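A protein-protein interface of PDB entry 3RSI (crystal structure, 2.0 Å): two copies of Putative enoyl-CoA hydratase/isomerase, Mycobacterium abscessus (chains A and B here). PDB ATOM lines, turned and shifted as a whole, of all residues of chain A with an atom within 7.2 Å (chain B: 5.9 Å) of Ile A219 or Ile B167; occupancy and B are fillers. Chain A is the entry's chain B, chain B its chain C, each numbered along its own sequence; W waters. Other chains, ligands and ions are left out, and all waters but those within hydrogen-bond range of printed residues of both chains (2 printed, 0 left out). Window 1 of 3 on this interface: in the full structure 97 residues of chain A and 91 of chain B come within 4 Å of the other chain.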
ATOM      1  N   ASP A 125      29.462   5.698 -19.573  1.00  0.00           N
ATOM      2  CA  ASP A 125      29.292   4.735 -20.677  1.00  0.00           C
ATOM      3  C   ASP A 125      29.189   3.294 -20.232  1.00  0.00           C
ATOM      4  O   ASP A 125      28.317   2.544 -20.701  1.00  0.00           O
ATOM      5  CB  ASP A 125      30.475   4.885 -21.625  1.00  0.00           C
ATOM      6  CG  ASP A 125      30.562   6.286 -22.175  1.00  0.00           C
ATOM      7  OD1 ASP A 125      29.519   6.777 -22.647  1.00  0.00           O
ATOM      8  OD2 ASP A 125      31.627   6.904 -22.104  1.00  0.00           O
ATOM      9  N   ASN A 207      42.615   0.065 -27.609  1.00  0.00           N
ATOM     10  CA  ASN A 207      41.825   0.241 -28.832  1.00  0.00           C
ATOM     11  C   ASN A 207      42.189   1.534 -29.554  1.00  0.00           C
ATOM     12  O   ASN A 207      42.785   2.441 -28.959  1.00  0.00           O
ATOM     13  CB  ASN A 207      40.332   0.189 -28.497  1.00  0.00           C
ATOM     14  CG  ASN A 207      39.933  -1.128 -27.843  1.00  0.00           C
ATOM     15  OD1 ASN A 207      40.660  -2.140 -27.939  1.00  0.00           O
ATOM     16  ND2 ASN A 207      38.780  -1.130 -27.179  1.00  0.00           N
ATOM     17  N   ALA A 211      38.909   5.656 -33.380  1.00  0.00           N
ATOM     18  CA  ALA A 211      37.828   4.678 -33.473  1.00  0.00           C
ATOM     19  C   ALA A 211      36.931   4.744 -32.245  1.00  0.00           C
ATOM     20  O   ALA A 211      35.725   4.829 -32.388  1.00  0.00           O
ATOM     21  CB  ALA A 211      38.376   3.297 -33.619  1.00  0.00           C
ATOM     22  N   VAL A 212      37.527   4.721 -31.053  1.00  0.00           N
ATOM     23  CA  VAL A 212      36.762   4.817 -29.797  1.00  0.00           C
ATOM     24  C   VAL A 212      35.993   6.150 -29.651  1.00  0.00           C
ATOM     25  O   VAL A 212      34.806   6.156 -29.324  1.00  0.00           O
ATOM     26  CB  VAL A 212      37.682   4.532 -28.565  1.00  0.00           C
ATOM     27  CG1 VAL A 212      36.959   4.844 -27.244  1.00  0.00           C
ATOM     28  CG2 VAL A 212      38.176   3.064 -28.613  1.00  0.00           C
ATOM     29  N   ARG A 213      36.661   7.280 -29.891  1.00  0.00           N
ATOM     30  CA  ARG A 213      36.014   8.604 -29.846  1.00  0.00           C
ATOM     31  C   ARG A 213      34.848   8.709 -30.857  1.00  0.00           C
ATOM     32  O   ARG A 213      33.736   9.100 -30.507  1.00  0.00           O
ATOM     33  CB  ARG A 213      37.073   9.679 -30.143  1.00  0.00           C
ATOM     34  CG  ARG A 213      36.564  11.074 -30.444  1.00  0.00           C
ATOM     35  CD  ARG A 213      37.709  12.072 -30.781  1.00  0.00           C
ATOM     36  NE  ARG A 213      38.901  11.779 -29.980  1.00  0.00           N
ATOM     37  CZ  ARG A 213      40.104  11.437 -30.455  1.00  0.00           C
ATOM     38  NH1 ARG A 213      41.091  11.171 -29.599  1.00  0.00           N
ATOM     39  NH2 ARG A 213      40.352  11.377 -31.761  1.00  0.00           N
ATOM     40  N   ASN A 214      35.104   8.364 -32.115  1.00  0.00           N
ATOM     41  CA  ASN A 214      34.050   8.478 -33.126  1.00  0.00           C
ATOM     42  C   ASN A 214      32.922   7.493 -32.899  1.00  0.00           C
ATOM     43  O   ASN A 214      31.765   7.807 -33.188  1.00  0.00           O
ATOM     44  CB  ASN A 214      34.591   8.371 -34.560  1.00  0.00           C
ATOM     45  CG  ASN A 214      35.360   9.617 -34.981  1.00  0.00           C
ATOM     46  OD1 ASN A 214      35.885  10.328 -34.136  1.00  0.00           O
ATOM     47  ND2 ASN A 214      35.432   9.875 -36.285  1.00  0.00           N
ATOM     48  N   ALA A 215      33.241   6.312 -32.378  1.00  0.00           N
ATOM     49  CA  ALA A 215      32.189   5.341 -32.047  1.00  0.00           C
ATOM     50  C   ALA A 215      31.264   5.871 -30.937  1.00  0.00           C
ATOM     51  O   ALA A 215      30.037   5.834 -31.062  1.00  0.00           O
ATOM     52  CB  ALA A 215      32.794   3.984 -31.668  1.00  0.00           C
ATOM     53  N   LYS A 216      31.844   6.371 -29.859  1.00  0.00           N
ATOM     54  CA  LYS A 216      31.027   6.988 -28.808  1.00  0.00           C
ATOM     55  C   LYS A 216      30.203   8.154 -29.343  1.00  0.00           C
ATOM     56  O   LYS A 216      29.028   8.260 -29.048  1.00  0.00           O
ATOM     57  CB  LYS A 216      31.869   7.454 -27.622  1.00  0.00           C
ATOM     58  CG  LYS A 216      30.998   8.099 -26.497  1.00  0.00           C
ATOM     59  CD  LYS A 216      31.796   8.483 -25.212  1.00  0.00           C
ATOM     60  CE  LYS A 216      30.891   9.245 -24.259  1.00  0.00           C
ATOM     61  NZ  LYS A 216      31.475   9.482 -22.906  1.00  0.00           N
ATOM     62  N   GLU A 217      30.804   9.007 -30.153  1.00  0.00           N
ATOM     63  CA  GLU A 217      30.100  10.166 -30.667  1.00  0.00           C
ATOM     64  C   GLU A 217      28.983   9.750 -31.607  1.00  0.00           C
ATOM     65  O   GLU A 217      27.905  10.361 -31.582  1.00  0.00           O
ATOM     66  CB  GLU A 217      31.061  11.132 -31.372  1.00  0.00           C
ATOM     67  CG  GLU A 217      30.354  12.388 -31.880  1.00  0.00           C
ATOM     68  CD  GLU A 217      31.300  13.419 -32.415  1.00  0.00           C
ATOM     69  OE1 GLU A 217      32.527  13.211 -32.365  1.00  0.00           O
ATOM     70  OE2 GLU A 217      30.802  14.447 -32.898  1.00  0.00           O
ATOM     71  N   ALA A 218      29.204   8.690 -32.402  1.00  0.00           N
ATOM     72  CA  ALA A 218      28.156   8.209 -33.330  1.00  0.00           C
ATOM     73  C   ALA A 218      26.984   7.590 -32.553  1.00  0.00           C
ATOM     74  O   ALA A 218      25.812   7.831 -32.862  1.00  0.00           O
ATOM     75  CB  ALA A 218      28.738   7.212 -34.384  1.00  0.00           C
ATOM     76  N   ILE A 219      27.319   6.811 -31.527  1.00  0.00           N
ATOM     77  CA  ILE A 219      26.318   6.212 -30.649  1.00  0.00           C
ATOM     78  C   ILE A 219      25.474   7.300 -29.987  1.00  0.00           C
ATOM     79  O   ILE A 219      24.252   7.236 -30.038  1.00  0.00           O
ATOM     80  CB  ILE A 219      26.968   5.325 -29.562  1.00  0.00           C
ATOM     81  CG1 ILE A 219      27.566   4.059 -30.187  1.00  0.00           C
ATOM     82  CG2 ILE A 219      25.968   4.918 -28.537  1.00  0.00           C
ATOM     83  CD1 ILE A 219      28.604   3.368 -29.279  1.00  0.00           C
ATOM     84  N   VAL A 220      26.122   8.304 -29.395  1.00  0.00           N
ATOM     85  CA  VAL A 220      25.392   9.357 -28.694  1.00  0.00           C
ATOM     86  C   VAL A 220      24.612  10.294 -29.615  1.00  0.00           C
ATOM     87  O   VAL A 220      23.423  10.532 -29.397  1.00  0.00           O
ATOM     88  CB  VAL A 220      26.312  10.187 -27.813  1.00  0.00           C
ATOM     89  CG1 VAL A 220      25.510  11.326 -27.174  1.00  0.00           C
ATOM     90  CG2 VAL A 220      26.993   9.281 -26.722  1.00  0.00           C
ATOM     91  N   ARG A 221      25.273  10.815 -30.641  1.00  0.00           N
ATOM     92  CA  ARG A 221      24.661  11.820 -31.498  1.00  0.00           C
ATOM     93  C   ARG A 221      23.592  11.247 -32.428  1.00  0.00           C
ATOM     94  O   ARG A 221      22.654  11.941 -32.749  1.00  0.00           O
ATOM     95  CB  ARG A 221      25.722  12.582 -32.303  1.00  0.00           C
ATOM     96  CG  ARG A 221      26.625  13.483 -31.451  1.00  0.00           C
ATOM     97  CD  ARG A 221      27.316  14.539 -32.339  1.00  0.00           C
ATOM     98  NE  ARG A 221      28.418  15.205 -31.641  1.00  0.00           N
ATOM     99  CZ  ARG A 221      28.290  16.202 -30.753  1.00  0.00           C
ATOM    100  NH1 ARG A 221      27.093  16.705 -30.431  1.00  0.00           N
ATOM    101  NH2 ARG A 221      29.381  16.713 -30.184  1.00  0.00           N
ATOM    102  N   SER A 222      23.702   9.979 -32.837  1.00  0.00           N
ATOM    103  CA  SER A 222      22.634   9.391 -33.661  1.00  0.00           C
ATOM    104  C   SER A 222      21.361   9.226 -32.863  1.00  0.00           C
ATOM    105  O   SER A 222      20.265   9.267 -33.432  1.00  0.00           O
ATOM    106  CB  SER A 222      23.028   8.049 -34.270  1.00  0.00           C
ATOM    107  OG  SER A 222      23.313   7.096 -33.289  1.00  0.00           O
ATOM    108  N   GLY A 223      21.511   9.031 -31.552  1.00  0.00           N
ATOM    109  CA  GLY A 223      20.374   8.952 -30.647  1.00  0.00           C
ATOM    110  C   GLY A 223      19.330   7.956 -31.113  1.00  0.00           C
ATOM    111  O   GLY A 223      19.656   6.876 -31.643  1.00  0.00           O
ATOM    112  N   TRP A 224      18.074   8.351 -30.939  1.00  0.00           N
ATOM    113  CA  TRP A 224      16.928   7.564 -31.363  1.00  0.00           C
ATOM    114  C   TRP A 224      16.210   8.303 -32.502  1.00  0.00           C
ATOM    115  O   TRP A 224      15.009   8.115 -32.734  1.00  0.00           O
ATOM    116  CB  TRP A 224      15.986   7.313 -30.162  1.00  0.00           C
ATOM    117  CG  TRP A 224      16.549   6.321 -29.127  1.00  0.00           C
ATOM    118  CD1 TRP A 224      16.170   5.033 -28.955  1.00  0.00           C
ATOM    119  CD2 TRP A 224      17.592   6.560 -28.164  1.00  0.00           C
ATOM    120  NE1 TRP A 224      16.901   4.442 -27.965  1.00  0.00           N
ATOM    121  CE2 TRP A 224      17.769   5.362 -27.441  1.00  0.00           C
ATOM    122  CE3 TRP A 224      18.371   7.673 -27.832  1.00  0.00           C
ATOM    123  CZ2 TRP A 224      18.703   5.233 -26.410  1.00  0.00           C
ATOM    124  CZ3 TRP A 224      19.306   7.549 -26.799  1.00  0.00           C
ATOM    125  CH2 TRP A 224      19.458   6.332 -26.099  1.00  0.00           C
ATOM    126  N   ILE A 233      24.476  10.507 -39.669  1.00  0.00           N
ATOM    127  CA  ILE A 233      25.359  10.891 -38.544  1.00  0.00           C
ATOM    128  C   ILE A 233      26.454   9.821 -38.355  1.00  0.00           C
ATOM    129  O   ILE A 233      27.654  10.127 -38.320  1.00  0.00           O
ATOM    130  CB  ILE A 233      24.541  11.094 -37.230  1.00  0.00           C
ATOM    131  CG1 ILE A 233      23.666  12.344 -37.335  1.00  0.00           C
ATOM    132  CG2 ILE A 233      25.444  11.180 -36.013  1.00  0.00           C
ATOM    133  CD1 ILE A 233      22.623  12.496 -36.198  1.00  0.00           C
ATOM    134  N   GLU A 234      26.029   8.566 -38.284  1.00  0.00           N
ATOM    135  CA  GLU A 234      26.948   7.429 -38.203  1.00  0.00           C
ATOM    136  C   GLU A 234      27.999   7.426 -39.339  1.00  0.00           C
ATOM    137  O   GLU A 234      29.188   7.232 -39.093  1.00  0.00           O
ATOM    138  CB  GLU A 234      26.146   6.127 -38.224  1.00  0.00           C
ATOM    139  CG  GLU A 234      27.000   4.848 -38.101  1.00  0.00           C
ATOM    140  CD  GLU A 234      26.134   3.606 -38.044  1.00  0.00           C
ATOM    141  OE1 GLU A 234      25.493   3.282 -39.076  1.00  0.00           O
ATOM    142  OE2 GLU A 234      26.056   2.989 -36.955  1.00  0.00           O
ATOM    143  N   LEU A 237      30.829  10.099 -39.118  1.00  0.00           N
ATOM    144  CA  LEU A 237      31.850   9.731 -38.123  1.00  0.00           C
ATOM    145  C   LEU A 237      32.604   8.432 -38.498  1.00  0.00           C
ATOM    146  O   LEU A 237      33.703   8.180 -38.022  1.00  0.00           O
ATOM    147  CB  LEU A 237      31.174   9.599 -36.745  1.00  0.00           C
ATOM    148  CG  LEU A 237      30.767  10.966 -36.161  1.00  0.00           C
ATOM    149  CD1 LEU A 237      29.642  10.895 -35.118  1.00  0.00           C
ATOM    150  CD2 LEU A 237      31.997  11.595 -35.541  1.00  0.00           C
ATOM    151  N   LEU B 137      31.440  -6.964 -31.162  1.00  0.00           N
ATOM    152  CA  LEU B 137      31.762  -6.009 -32.208  1.00  0.00           C
ATOM    153  C   LEU B 137      33.190  -5.511 -31.943  1.00  0.00           C
ATOM    154  O   LEU B 137      33.361  -4.461 -31.353  1.00  0.00           O
ATOM    155  CB  LEU B 137      30.751  -4.853 -32.183  1.00  0.00           C
ATOM    156  CG  LEU B 137      29.302  -5.193 -32.502  1.00  0.00           C
ATOM    157  CD1 LEU B 137      28.337  -4.084 -32.066  1.00  0.00           C
ATOM    158  CD2 LEU B 137      29.146  -5.504 -34.010  1.00  0.00           C
ATOM    159  N   VAL B 140      36.811  -1.725 -32.902  1.00  0.00           N
ATOM    160  CA  VAL B 140      37.691  -0.731 -32.272  1.00  0.00           C
ATOM    161  C   VAL B 140      39.069  -1.278 -31.900  1.00  0.00           C
ATOM    162  O   VAL B 140      40.052  -0.511 -31.816  1.00  0.00           O
ATOM    163  CB  VAL B 140      37.046  -0.069 -31.004  1.00  0.00           C
ATOM    164  CG1 VAL B 140      35.857   0.822 -31.412  1.00  0.00           C
ATOM    165  CG2 VAL B 140      36.646  -1.127 -29.952  1.00  0.00           C
ATOM    166  N   PRO B 146      32.108  -0.374 -35.872  1.00  0.00           N
ATOM    167  CA  PRO B 146      31.000  -1.109 -36.463  1.00  0.00           C
ATOM    168  C   PRO B 146      30.002  -0.129 -37.092  1.00  0.00           C
ATOM    169  O   PRO B 146      28.989   0.224 -36.481  1.00  0.00           O
ATOM    170  CB  PRO B 146      30.406  -1.842 -35.268  1.00  0.00           C
ATOM    171  CG  PRO B 146      30.665  -0.934 -34.113  1.00  0.00           C
ATOM    172  CD  PRO B 146      31.941  -0.194 -34.422  1.00  0.00           C
ATOM    173  N   SER B 150      25.396  -0.370 -36.296  1.00  0.00           N
ATOM    174  CA  SER B 150      25.430  -0.761 -34.885  1.00  0.00           C
ATOM    175  C   SER B 150      25.427   0.429 -33.946  1.00  0.00           C
ATOM    176  O   SER B 150      24.877   0.353 -32.839  1.00  0.00           O
ATOM    177  CB  SER B 150      26.645  -1.635 -34.572  1.00  0.00           C
ATOM    178  OG  SER B 150      26.529  -2.898 -35.198  1.00  0.00           O
ATOM    179  N   MET B 151      26.058   1.522 -34.362  1.00  0.00           N
ATOM    180  CA  MET B 151      26.160   2.686 -33.490  1.00  0.00           C
ATOM    181  C   MET B 151      24.813   3.407 -33.390  1.00  0.00           C
ATOM    182  O   MET B 151      24.458   3.904 -32.322  1.00  0.00           O
ATOM    183  CB  MET B 151      27.327   3.586 -33.893  1.00  0.00           C
ATOM    184  CG  MET B 151      28.671   2.824 -33.729  1.00  0.00           C
ATOM    185  SD  MET B 151      30.109   3.669 -34.360  1.00  0.00           S
ATOM    186  CE  MET B 151      29.778   3.543 -36.106  1.00  0.00           C
ATOM    187  N   VAL B 152      24.052   3.384 -34.484  1.00  0.00           N
ATOM    188  CA  VAL B 152      22.665   3.848 -34.496  1.00  0.00           C
ATOM    189  C   VAL B 152      21.794   2.947 -33.600  1.00  0.00           C
ATOM    190  O   VAL B 152      21.125   3.435 -32.660  1.00  0.00           O
ATOM    191  CB  VAL B 152      22.055   3.850 -35.922  1.00  0.00           C
ATOM    192  CG1 VAL B 152      20.485   4.006 -35.878  1.00  0.00           C
ATOM    193  CG2 VAL B 152      22.703   4.961 -36.811  1.00  0.00           C
ATOM    194  N   LEU B 154      22.268  -0.382 -31.770  1.00  0.00           N
ATOM    195  CA  LEU B 154      22.484  -1.329 -30.651  1.00  0.00           C
ATOM    196  C   LEU B 154      21.915  -0.805 -29.324  1.00  0.00           C
ATOM    197  O   LEU B 154      21.185  -1.539 -28.613  1.00  0.00           O
ATOM    198  CB  LEU B 154      23.960  -1.721 -30.504  1.00  0.00           C
ATOM    199  CG  LEU B 154      24.283  -2.867 -29.526  1.00  0.00           C
ATOM    200  CD1 LEU B 154      23.623  -4.195 -29.953  1.00  0.00           C
ATOM    201  CD2 LEU B 154      25.846  -3.021 -29.395  1.00  0.00           C
ATOM    202  N   LYS B 155      22.173   0.467 -29.025  1.00  0.00           N
ATOM    203  CA  LYS B 155      21.610   1.100 -27.817  1.00  0.00           C
ATOM    204  C   LYS B 155      20.070   1.201 -27.823  1.00  0.00           C
ATOM    205  O   LYS B 155      19.461   1.346 -26.760  1.00  0.00           O
ATOM    206  CB  LYS B 155      22.192   2.495 -27.635  1.00  0.00           C
ATOM    207  CG  LYS B 155      21.724   3.458 -28.721  1.00  0.00           C
ATOM    208  CD  LYS B 155      22.311   4.800 -28.566  1.00  0.00           C
ATOM    209  CE  LYS B 155      21.615   5.780 -29.521  1.00  0.00           C
ATOM    210  NZ  LYS B 155      22.078   5.548 -30.928  1.00  0.00           N
ATOM    211  N   TYR B 160      21.521   0.663 -22.850  1.00  0.00           N
ATOM    212  CA  TYR B 160      22.499   1.634 -23.286  1.00  0.00           C
ATOM    213  C   TYR B 160      23.892   1.299 -22.791  1.00  0.00           C
ATOM    214  O   TYR B 160      24.819   1.223 -23.588  1.00  0.00           O
ATOM    215  CB  TYR B 160      22.068   3.007 -22.749  1.00  0.00           C
ATOM    216  CG  TYR B 160      22.986   4.174 -23.063  1.00  0.00           C
ATOM    217  CD1 TYR B 160      22.844   4.895 -24.252  1.00  0.00           C
ATOM    218  CD2 TYR B 160      23.936   4.606 -22.155  1.00  0.00           C
ATOM    219  CE1 TYR B 160      23.636   5.992 -24.536  1.00  0.00           C
ATOM    220  CE2 TYR B 160      24.746   5.740 -22.432  1.00  0.00           C
ATOM    221  CZ  TYR B 160      24.581   6.407 -23.639  1.00  0.00           C
ATOM    222  OH  TYR B 160      25.342   7.504 -23.950  1.00  0.00           O
ATOM    223  N   LYS B 162      25.268  -1.524 -21.824  1.00  0.00           N
ATOM    224  CA  LYS B 162      25.916  -2.709 -22.429  1.00  0.00           C
ATOM    225  C   LYS B 162      26.217  -2.505 -23.918  1.00  0.00           C
ATOM    226  O   LYS B 162      27.226  -3.019 -24.429  1.00  0.00           O
ATOM    227  CB  LYS B 162      25.109  -3.978 -22.214  1.00  0.00           C
ATOM    228  CG  LYS B 162      26.013  -5.208 -22.087  1.00  0.00           C
ATOM    229  CD  LYS B 162      26.687  -5.210 -20.704  1.00  0.00           C
ATOM    230  CE  LYS B 162      27.725  -6.248 -20.567  1.00  0.00           C
ATOM    231  NZ  LYS B 162      28.567  -6.042 -19.349  1.00  0.00           N
ATOM    232  N   ALA B 163      25.364  -1.740 -24.605  1.00  0.00           N
ATOM    233  CA  ALA B 163      25.638  -1.352 -26.002  1.00  0.00           C
ATOM    234  C   ALA B 163      26.940  -0.558 -26.079  1.00  0.00           C
ATOM    235  O   ALA B 163      27.813  -0.829 -26.918  1.00  0.00           O
ATOM    236  CB  ALA B 163      24.464  -0.555 -26.608  1.00  0.00           C
ATOM    237  N   MET B 164      27.091   0.399 -25.172  1.00  0.00           N
ATOM    238  CA  MET B 164      28.302   1.205 -25.117  1.00  0.00           C
ATOM    239  C   MET B 164      29.506   0.358 -24.837  1.00  0.00           C
ATOM    240  O   MET B 164      30.514   0.507 -25.490  1.00  0.00           O
ATOM    241  CB  MET B 164      28.239   2.237 -24.011  1.00  0.00           C
ATOM    242  CG  MET B 164      27.707   3.529 -24.422  1.00  0.00           C
ATOM    243  SD  MET B 164      28.670   4.414 -25.637  1.00  0.00           S
ATOM    244  CE  MET B 164      27.754   5.960 -25.506  1.00  0.00           C
ATOM    245  N   GLU B 165      29.387  -0.513 -23.846  1.00  0.00           N
ATOM    246  CA  GLU B 165      30.472  -1.405 -23.445  1.00  0.00           C
ATOM    247  C   GLU B 165      30.911  -2.284 -24.599  1.00  0.00           C
ATOM    248  O   GLU B 165      32.107  -2.408 -24.879  1.00  0.00           O
ATOM    249  CB  GLU B 165      30.070  -2.269 -22.251  1.00  0.00           C
ATOM    250  CG  GLU B 165      31.252  -3.072 -21.702  1.00  0.00           C
ATOM    251  CD  GLU B 165      30.919  -3.850 -20.464  1.00  0.00           C
ATOM    252  OE1 GLU B 165      29.817  -3.668 -19.916  1.00  0.00           O
ATOM    253  OE2 GLU B 165      31.766  -4.664 -20.042  1.00  0.00           O
ATOM    254  N   MET B 166      29.947  -2.894 -25.275  1.00  0.00           N
ATOM    255  CA  MET B 166      30.272  -3.780 -26.394  1.00  0.00           C
ATOM    256  C   MET B 166      31.099  -3.046 -27.470  1.00  0.00           C
ATOM    257  O   MET B 166      32.121  -3.560 -27.941  1.00  0.00           O
ATOM    258  CB  MET B 166      29.014  -4.373 -26.990  1.00  0.00           C
ATOM    259  CG  MET B 166      28.417  -5.515 -26.203  1.00  0.00           C
ATOM    260  SD  MET B 166      26.899  -6.101 -26.977  1.00  0.00           S
ATOM    261  CE  MET B 166      27.580  -6.915 -28.428  1.00  0.00           C
ATOM    262  N   ILE B 167      30.656  -1.851 -27.865  1.00  0.00           N
ATOM    263  CA  ILE B 167      31.274  -1.139 -29.005  1.00  0.00           C
ATOM    264  C   ILE B 167      32.602  -0.489 -28.611  1.00  0.00           C
ATOM    265  O   ILE B 167      33.572  -0.521 -29.367  1.00  0.00           O
ATOM    266  CB  ILE B 167      30.275  -0.090 -29.626  1.00  0.00           C
ATOM    267  CG1 ILE B 167      29.058  -0.845 -30.155  1.00  0.00           C
ATOM    268  CG2 ILE B 167      30.916   0.740 -30.778  1.00  0.00           C
ATOM    269  CD1 ILE B 167      27.943   0.001 -30.744  1.00  0.00           C
ATOM    270  N   LEU B 168      32.650   0.081 -27.422  1.00  0.00           N
ATOM    271  CA  LEU B 168      33.839   0.783 -26.976  1.00  0.00           C
ATOM    272  C   LEU B 168      34.960  -0.149 -26.527  1.00  0.00           C
ATOM    273  O   LEU B 168      36.113   0.171 -26.765  1.00  0.00           O
ATOM    274  CB  LEU B 168      33.504   1.797 -25.880  1.00  0.00           C
ATOM    275  CG  LEU B 168      32.548   2.934 -26.248  1.00  0.00           C
ATOM    276  CD1 LEU B 168      32.522   4.021 -25.178  1.00  0.00           C
ATOM    277  CD2 LEU B 168      32.912   3.560 -27.614  1.00  0.00           C
ATOM    278  N   THR B 169      34.646  -1.288 -25.903  1.00  0.00           N
ATOM    279  CA  THR B 169      35.686  -2.240 -25.479  1.00  0.00           C
ATOM    280  C   THR B 169      36.012  -3.227 -26.575  1.00  0.00           C
ATOM    281  O   THR B 169      37.158  -3.658 -26.688  1.00  0.00           O
ATOM    282  CB  THR B 169      35.298  -3.090 -24.237  1.00  0.00           C
ATOM    283  OG1 THR B 169      34.277  -4.043 -24.598  1.00  0.00           O
ATOM    284  CG2 THR B 169      34.848  -2.202 -23.071  1.00  0.00           C
ATOM    285  N   GLY B 170      35.009  -3.571 -27.378  1.00  0.00           N
ATOM    286  CA  GLY B 170      35.151  -4.579 -28.415  1.00  0.00           C
ATOM    287  C   GLY B 170      35.056  -6.019 -27.927  1.00  0.00           C
ATOM    288  O   GLY B 170      35.277  -6.962 -28.711  1.00  0.00           O
HETATM  289  O   HOH W   1      16.460   2.397 -25.895  1.00  0.00           O
HETATM  290  O   HOH W   2      27.292   7.993 -22.169  1.00  0.00           O
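Water W2 lies within hydrogen-bond range of OD1 of Asp A125 (2.6 Å) and OH of Tyr B160 (2.7 Å).
Water W1 bridges the indole nitrogen (NE1) of Trp A224 (2.9 Å) and the backbone carbonyl oxygen (O) of Lys B155 (3.3 Å).
No position is printed for both chains.
Of the 24 pairs that touch across the chains among the printed residues, none has its exchanged pair printed and touching as well.
Among the printed residues, merely in contact across the chains: Asp A125 with Met B164, Asn A207 with Val B140, Val A212 with Leu B168, Ala A215 with Met B151, Ala A215 with Ile B167, Lys A216 with Leu B168, Ala A218 with Met B151, Ile A219 with Met B151, Ile A219 with Met B164, Ile A219 with Ile B167, Val A220 with Tyr B160, Val A220 with Met B164, Ser A222 with Met B151, Ser A222 with Val B152, Gly A223 with Val B152 and Trp A224 with Lys B155.
OG of Ser A222 lies within hydrogen-bond range of NZ of Lys B155, at 3.1 Å.
The backbone carbonyl oxygen (O) of Gly A223 sits at hydrogen-bond distance from the side-chain amino group (NZ) of Lys B155, 2.9 Å away.
The side-chain carboxylate (OE2) of Glu A234 lies within hydrogen-bond range of the backbone NH (N) of Val B152 (3.2 Å).
The backbone carbonyl oxygen of Ile A219 is in hydrogen-bond range of the side-chain amino group of Lys B155.
O of Thr B169 sits at hydrogen-bond distance from ND2 of Asn A207.
OE2 of Glu A234 sits at hydrogen-bond distance from N of Met B151 (3.0 Å).
The side-chain carboxylate (OE2) of Glu A234 is in hydrogen-bond range of the backbone NH (N) of Ser B150, at 3.5 Å.
ND2 of Asn A207 lies within hydrogen-bond range of O of Leu B168 (3.0 Å).
The side-chain carboxylate of Asp A125 lies within salt-bridge range of the side-chain amino group of Lys A216 (2.7 Å).
The side-chain amino group of Lys B155 sits at hydrogen-bond distance from the backbone carbonyl oxygen of Val B152, at 2.9 Å.
O of Ile A219 is in hydrogen-bond range of OG of Ser A222.
O of Glu B165 is in hydrogen-bond range of OG1 of Thr B169.
NZ of Lys B155 is in hydrogen-bond range of O of Met B151, at 3.2 Å.
O of Ala A218 is in hydrogen-bond range of OG of Ser A222 (2.6 Å).
Hydrophobic or aromatic side chains of chain A that line the printed part of chain B: Ala A215, Ala A218, Ile A219, Val A220 and Trp A224.
Of the 18 printed residues of chain B, 10 touch a printed residue of chain A.
Among the printed residues, 24 pairs touch across the chains.
Among the printed residues, no Asp or Glu carboxylate lies within 4 Å of a Lys or Arg side-chain nitrogen of the other chain.
Of the printed residues of chain B, Lys A216 touches Leu B168.
Of chain B, only Met B151 (3.4 Å), Lys B155 (2.9 Å), Met B164 (3.7 Å) and Ile B167 (3.7 Å) come within 4 Å of Ile A219.
Of the printed residues of chain A, Val B140 touches Asn A207.
Of the printed residues of chain A, Tyr B160 touches Val A220.
Of chain A, only Ala A215 and Ile A219 come within 4 Å of Ile B167.
The nearest residue of chain A that does not touch Ile B167 is Asn A207 (5.7 Å).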
